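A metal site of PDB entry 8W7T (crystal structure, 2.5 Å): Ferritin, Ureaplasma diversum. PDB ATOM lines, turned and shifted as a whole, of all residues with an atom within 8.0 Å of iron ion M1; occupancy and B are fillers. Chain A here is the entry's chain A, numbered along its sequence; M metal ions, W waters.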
ATOM      1  N   ASN A  27       9.854 -22.277   3.708  1.00  0.00           N
ATOM      2  CA  ASN A  27      10.058 -22.073   2.302  1.00  0.00           C
ATOM      3  C   ASN A  27       9.469 -20.794   1.768  1.00  0.00           C
ATOM      4  O   ASN A  27      10.053 -20.150   0.941  1.00  0.00           O
ATOM      5  CB  ASN A  27       9.560 -23.276   1.560  1.00  0.00           C
ATOM      6  CG  ASN A  27      10.604 -24.345   1.441  1.00  0.00           C
ATOM      7  OD1 ASN A  27      11.550 -24.181   0.711  1.00  0.00           O
ATOM      8  ND2 ASN A  27      10.446 -25.432   2.159  1.00  0.00           N
ATOM      9  N   HIS A  56      16.405 -17.098  -8.468  1.00  0.00           N
ATOM     10  CA  HIS A  56      16.005 -18.402  -8.912  1.00  0.00           C
ATOM     11  C   HIS A  56      15.833 -19.313  -7.757  1.00  0.00           C
ATOM     12  O   HIS A  56      14.883 -20.068  -7.724  1.00  0.00           O
ATOM     13  CB  HIS A  56      16.959 -18.927  -9.971  1.00  0.00           C
ATOM     14  CG  HIS A  56      16.835 -18.212 -11.276  1.00  0.00           C
ATOM     15  ND1 HIS A  56      17.790 -18.263 -12.255  1.00  0.00           N
ATOM     16  CD2 HIS A  56      15.863 -17.391 -11.740  1.00  0.00           C
ATOM     17  CE1 HIS A  56      17.422 -17.519 -13.275  1.00  0.00           C
ATOM     18  NE2 HIS A  56      16.256 -16.979 -13.001  1.00  0.00           N
ATOM     19  N   LEU A  57      16.543 -19.039  -6.673  1.00  0.00           N
ATOM     20  CA  LEU A  57      16.385 -19.830  -5.475  1.00  0.00           C
ATOM     21  C   LEU A  57      15.117 -19.367  -4.751  1.00  0.00           C
ATOM     22  O   LEU A  57      14.449 -20.162  -4.164  1.00  0.00           O
ATOM     23  CB  LEU A  57      17.615 -19.706  -4.616  1.00  0.00           C
ATOM     24  CG  LEU A  57      17.869 -20.680  -3.474  1.00  0.00           C
ATOM     25  CD1 LEU A  57      17.939 -22.109  -3.986  1.00  0.00           C
ATOM     26  CD2 LEU A  57      19.164 -20.298  -2.799  1.00  0.00           C
ATOM     27  N   GLU A  59      12.397 -18.356  -6.200  1.00  0.00           N
ATOM     28  CA  GLU A  59      11.324 -18.950  -6.927  1.00  0.00           C
ATOM     29  C   GLU A  59      11.239 -20.442  -6.738  1.00  0.00           C
ATOM     30  O   GLU A  59      10.180 -21.001  -6.894  1.00  0.00           O
ATOM     31  CB  GLU A  59      11.499 -18.594  -8.374  1.00  0.00           C
ATOM     32  CG  GLU A  59      11.285 -17.142  -8.707  1.00  0.00           C
ATOM     33  CD  GLU A  59      11.977 -16.738  -9.980  1.00  0.00           C
ATOM     34  OE1 GLU A  59      11.894 -15.568 -10.363  1.00  0.00           O
ATOM     35  OE2 GLU A  59      12.615 -17.607 -10.606  1.00  0.00           O
ATOM     36  N   ASP A  60      12.334 -21.088  -6.398  1.00  0.00           N
ATOM     37  CA  ASP A  60      12.329 -22.492  -6.099  1.00  0.00           C
ATOM     38  C   ASP A  60      11.626 -22.722  -4.767  1.00  0.00           C
ATOM     39  O   ASP A  60      10.802 -23.587  -4.655  1.00  0.00           O
ATOM     40  CB  ASP A  60      13.765 -22.992  -6.090  1.00  0.00           C
ATOM     41  CG  ASP A  60      13.872 -24.435  -5.889  1.00  0.00           C
ATOM     42  OD1 ASP A  60      13.124 -25.134  -6.578  1.00  0.00           O
ATOM     43  OD2 ASP A  60      14.718 -24.868  -5.071  1.00  0.00           O
ATOM     44  N   LYS A  61      11.932 -21.903  -3.786  1.00  0.00           N
ATOM     45  CA  LYS A  61      11.336 -22.041  -2.469  1.00  0.00           C
ATOM     46  C   LYS A  61       9.865 -21.680  -2.436  1.00  0.00           C
ATOM     47  O   LYS A  61       9.107 -22.314  -1.744  1.00  0.00           O
ATOM     48  CB  LYS A  61      12.112 -21.245  -1.433  1.00  0.00           C
ATOM     49  CG  LYS A  61      13.606 -21.433  -1.349  1.00  0.00           C
ATOM     50  CD  LYS A  61      14.004 -22.881  -1.171  1.00  0.00           C
ATOM     51  CE  LYS A  61      15.500 -22.988  -1.023  1.00  0.00           C
ATOM     52  NZ  LYS A  61      15.925 -24.343  -0.593  1.00  0.00           N
ATOM     53  N   VAL A  64       7.948 -25.024  -6.145  1.00  0.00           N
ATOM     54  CA  VAL A  64       7.881 -26.435  -5.906  1.00  0.00           C
ATOM     55  C   VAL A  64       8.048 -26.892  -4.479  1.00  0.00           C
ATOM     56  O   VAL A  64       7.376 -27.775  -4.035  1.00  0.00           O
ATOM     57  CB  VAL A  64       8.831 -27.189  -6.834  1.00  0.00           C
ATOM     58  CG1 VAL A  64       8.307 -27.165  -8.257  1.00  0.00           C
ATOM     59  CG2 VAL A  64      10.242 -26.654  -6.768  1.00  0.00           C
ATOM     60  N   HIS A  65       8.901 -26.233  -3.739  1.00  0.00           N
ATOM     61  CA  HIS A  65       9.120 -26.561  -2.363  1.00  0.00           C
ATOM     62  C   HIS A  65       7.878 -26.443  -1.518  1.00  0.00           C
ATOM     63  O   HIS A  65       7.666 -27.228  -0.639  1.00  0.00           O
ATOM     64  CB  HIS A  65      10.207 -25.685  -1.836  1.00  0.00           C
ATOM     65  CG  HIS A  65      11.588 -26.147  -2.150  1.00  0.00           C
ATOM     66  ND1 HIS A  65      12.426 -26.673  -1.195  1.00  0.00           N
ATOM     67  CD2 HIS A  65      12.296 -26.110  -3.295  1.00  0.00           C
ATOM     68  CE1 HIS A  65      13.590 -26.967  -1.751  1.00  0.00           C
ATOM     69  NE2 HIS A  65      13.533 -26.630  -3.022  1.00  0.00           N
ATOM     70  N   GLU A 106      20.542 -22.471   4.160  1.00  0.00           N
ATOM     71  CA  GLU A 106      20.338 -23.718   3.432  1.00  0.00           C
ATOM     72  C   GLU A 106      20.844 -24.927   4.179  1.00  0.00           C
ATOM     73  O   GLU A 106      20.390 -26.015   3.962  1.00  0.00           O
ATOM     74  CB  GLU A 106      20.972 -23.648   2.054  1.00  0.00           C
ATOM     75  CG  GLU A 106      20.385 -22.628   1.103  1.00  0.00           C
ATOM     76  CD  GLU A 106      18.970 -22.948   0.706  1.00  0.00           C
ATOM     77  OE1 GLU A 106      18.723 -24.073   0.269  1.00  0.00           O
ATOM     78  OE2 GLU A 106      18.124 -22.073   0.838  1.00  0.00           O
ATOM     79  N   VAL A 109      18.157 -25.853   6.426  1.00  0.00           N
ATOM     80  CA  VAL A 109      17.111 -26.569   5.737  1.00  0.00           C
ATOM     81  C   VAL A 109      17.395 -28.045   5.840  1.00  0.00           C
ATOM     82  O   VAL A 109      16.532 -28.834   6.124  1.00  0.00           O
ATOM     83  CB  VAL A 109      16.996 -26.105   4.262  1.00  0.00           C
ATOM     84  CG1 VAL A 109      16.337 -27.142   3.379  1.00  0.00           C
ATOM     85  CG2 VAL A 109      16.283 -24.778   4.176  1.00  0.00           C
ATOM     86  N   TRP A 134      12.651 -36.460  -1.682  1.00  0.00           N
ATOM     87  CA  TRP A 134      12.884 -35.349  -2.594  1.00  0.00           C
ATOM     88  C   TRP A 134      13.595 -34.211  -1.888  1.00  0.00           C
ATOM     89  O   TRP A 134      14.564 -33.641  -2.414  1.00  0.00           O
ATOM     90  CB  TRP A 134      11.544 -34.857  -3.182  1.00  0.00           C
ATOM     91  CG  TRP A 134      11.741 -33.865  -4.293  1.00  0.00           C
ATOM     92  CD1 TRP A 134      11.880 -34.147  -5.617  1.00  0.00           C
ATOM     93  CD2 TRP A 134      11.850 -32.428  -4.180  1.00  0.00           C
ATOM     94  NE1 TRP A 134      12.053 -32.989  -6.335  1.00  0.00           N
ATOM     95  CE2 TRP A 134      12.046 -31.920  -5.479  1.00  0.00           C
ATOM     96  CE3 TRP A 134      11.788 -31.531  -3.100  1.00  0.00           C
ATOM     97  CZ2 TRP A 134      12.191 -30.542  -5.749  1.00  0.00           C
ATOM     98  CZ3 TRP A 134      11.933 -30.153  -3.369  1.00  0.00           C
ATOM     99  CH2 TRP A 134      12.133 -29.681  -4.678  1.00  0.00           C
ATOM    100  N   TYR A 135      13.155 -33.871  -0.682  1.00  0.00           N
ATOM    101  CA  TYR A 135      13.714 -32.747   0.044  1.00  0.00           C
ATOM    102  C   TYR A 135      15.055 -33.095   0.658  1.00  0.00           C
ATOM    103  O   TYR A 135      15.936 -32.231   0.759  1.00  0.00           O
ATOM    104  CB  TYR A 135      12.732 -32.279   1.118  1.00  0.00           C
ATOM    105  CG  TYR A 135      11.459 -31.668   0.559  1.00  0.00           C
ATOM    106  CD1 TYR A 135      10.442 -32.461   0.052  1.00  0.00           C
ATOM    107  CD2 TYR A 135      11.270 -30.280   0.561  1.00  0.00           C
ATOM    108  CE1 TYR A 135       9.266 -31.911  -0.449  1.00  0.00           C
ATOM    109  CE2 TYR A 135      10.097 -29.717   0.064  1.00  0.00           C
ATOM    110  CZ  TYR A 135       9.106 -30.546  -0.442  1.00  0.00           C
ATOM    111  OH  TYR A 135       7.932 -30.006  -0.939  1.00  0.00           O
ATOM    112  N   ARG A 137      17.261 -35.058  -0.853  1.00  0.00           N
ATOM    113  CA  ARG A 137      18.143 -34.839  -1.996  1.00  0.00           C
ATOM    114  C   ARG A 137      18.316 -33.354  -2.297  1.00  0.00           C
ATOM    115  O   ARG A 137      19.444 -32.869  -2.498  1.00  0.00           O
ATOM    116  CB  ARG A 137      17.603 -35.584  -3.218  1.00  0.00           C
ATOM    117  CG  ARG A 137      18.424 -35.363  -4.484  1.00  0.00           C
ATOM    118  CD  ARG A 137      17.575 -35.463  -5.763  1.00  0.00           C
ATOM    119  NE  ARG A 137      16.311 -34.709  -5.697  1.00  0.00           N
ATOM    120  CZ  ARG A 137      16.212 -33.382  -5.804  1.00  0.00           C
ATOM    121  NH1 ARG A 137      17.285 -32.622  -5.971  1.00  0.00           N
ATOM    122  NH2 ARG A 137      15.017 -32.814  -5.724  1.00  0.00           N
ATOM    123  N   ASP A 138      17.210 -32.597  -2.337  1.00  0.00           N
ATOM    124  CA  ASP A 138      17.317 -31.195  -2.718  1.00  0.00           C
ATOM    125  C   ASP A 138      18.044 -30.362  -1.664  1.00  0.00           C
ATOM    126  O   ASP A 138      18.608 -29.309  -1.993  1.00  0.00           O
ATOM    127  CB  ASP A 138      15.936 -30.617  -2.995  1.00  0.00           C
ATOM    128  CG  ASP A 138      15.979 -29.410  -3.923  1.00  0.00           C
ATOM    129  OD1 ASP A 138      16.099 -29.593  -5.148  1.00  0.00           O
ATOM    130  OD2 ASP A 138      15.895 -28.280  -3.401  1.00  0.00           O
ATOM    131  N   GLY A 139      18.018 -30.790  -0.397  1.00  0.00           N
ATOM    132  CA  GLY A 139      18.780 -30.092   0.626  1.00  0.00           C
ATOM    133  C   GLY A 139      20.258 -30.016   0.285  1.00  0.00           C
ATOM    134  O   GLY A 139      20.889 -28.970   0.467  1.00  0.00           O
ATOM    135  N   LYS A 141      21.527 -30.641  -2.904  1.00  0.00           N
ATOM    136  CA  LYS A 141      21.634 -29.982  -4.208  1.00  0.00           C
ATOM    137  C   LYS A 141      21.659 -28.471  -4.043  1.00  0.00           C
ATOM    138  O   LYS A 141      22.559 -27.795  -4.562  1.00  0.00           O
ATOM    139  CB  LYS A 141      20.470 -30.395  -5.117  1.00  0.00           C
ATOM    140  CG  LYS A 141      20.626 -29.997  -6.588  1.00  0.00           C
ATOM    141  CD  LYS A 141      19.961 -28.649  -6.886  1.00  0.00           C
ATOM    142  CE  LYS A 141      18.438 -28.751  -7.011  1.00  0.00           C
ATOM    143  NZ  LYS A 141      17.788 -27.403  -7.004  1.00  0.00           N
ATOM    144  N   ASP A 142      20.670 -27.922  -3.329  1.00  0.00           N
ATOM    145  CA  ASP A 142      20.604 -26.470  -3.195  1.00  0.00           C
ATOM    146  C   ASP A 142      21.797 -25.937  -2.428  1.00  0.00           C
ATOM    147  O   ASP A 142      22.363 -24.890  -2.771  1.00  0.00           O
ATOM    148  CB  ASP A 142      19.296 -26.060  -2.520  1.00  0.00           C
ATOM    149  CG  ASP A 142      18.100 -26.064  -3.468  1.00  0.00           C
ATOM    150  OD1 ASP A 142      18.302 -26.277  -4.686  1.00  0.00           O
ATOM    151  OD2 ASP A 142      16.956 -25.851  -2.995  1.00  0.00           O
ATOM    152  N   LEU A 143      22.218 -26.666  -1.376  1.00  0.00           N
ATOM    153  CA  LEU A 143      23.389 -26.248  -0.634  1.00  0.00           C
ATOM    154  C   LEU A 143      24.631 -26.237  -1.516  1.00  0.00           C
ATOM    155  O   LEU A 143      25.476 -25.327  -1.415  1.00  0.00           O
ATOM    156  CB  LEU A 143      23.617 -27.168   0.553  1.00  0.00           C
ATOM    157  CG  LEU A 143      24.773 -26.647   1.401  1.00  0.00           C
ATOM    158  CD1 LEU A 143      24.255 -25.593   2.389  1.00  0.00           C
ATOM    159  CD2 LEU A 143      25.540 -27.780   2.100  1.00  0.00           C
ATOM    160  N   GLU A 145      24.785 -25.813  -4.847  1.00  0.00           N
ATOM    161  CA  GLU A 145      24.701 -24.678  -5.754  1.00  0.00           C
ATOM    162  C   GLU A 145      25.137 -23.412  -5.058  1.00  0.00           C
ATOM    163  O   GLU A 145      25.957 -22.640  -5.584  1.00  0.00           O
ATOM    164  CB  GLU A 145      23.280 -24.538  -6.302  1.00  0.00           C
ATOM    165  CG  GLU A 145      22.847 -25.652  -7.268  1.00  0.00           C
ATOM    166  CD  GLU A 145      21.401 -25.511  -7.767  1.00  0.00           C
ATOM    167  OE1 GLU A 145      20.618 -24.745  -7.158  1.00  0.00           O
ATOM    168  OE2 GLU A 145      21.053 -26.163  -8.774  1.00  0.00           O
HETATM  169 FE    FE M   1      15.498 -26.578  -4.444  1.00  0.00          FE
HETATM  170 FE    FE M   2      17.995 -25.025  -9.818  1.00  0.00          FE
HETATM  171  O   HOH W   1      14.694 -27.418  -6.496  1.00  0.00           O
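Residues that only touch iron ion M1: Lys 141 (3.5 Å). Five residues have an atom within 4 Å of iron ion M1: Asp 60, His 65, Asp 138, Lys 141 and Asp 142.
Iron ion M1 is bound by the side-chain carboxylate of Asp 60 (2.0 Å), the side-chain carboxylate of Asp 138 (2.0 Å), the side-chain carboxylate of Asp 142 (2.2 Å), water W1 (2.4 Å) and a ring nitrogen (NE2) of His 65 (2.4 Å). Slightly farther from iron ion M1 lies OD1 of Asp 142 (2.8 Å).
Water W1 lies within hydrogen-bond range of the side-chain carboxylate (OD1) of Asp 60 (2.8 Å), the side-chain carboxylate (OD1) of Asp 138 (2.9 Å) and the side-chain amino group (NZ) of Lys 141 (3.1 Å).
NZ of Lys 141 lies within salt-bridge range of OD1 of Asp 138. The side-chain carboxylate of Asp 138 lies within salt-bridge range of the guanidinium group of Arg 137 (3.4 Å). The side-chain carboxylate (OD1) of Asp 142 is in salt-bridge range of the side-chain amino group (NZ) of Lys 141, at 2.6 Å. The side-chain carboxylate (OD2) of Asp 142 sits close to the side-chain amino group (NZ) of Lys 61 (3.0 Å). OD1 of Asn 27 lies close to ND1 of His 65, 3.3 Å away. The side-chain hydroxyl of Tyr 135 lies within hydrogen-bond range of the backbone carbonyl oxygen of His 65. The side-chain amino group of Lys 141 lies within salt-bridge range of the side-chain carboxylate of Glu 145, 3.9 Å away.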
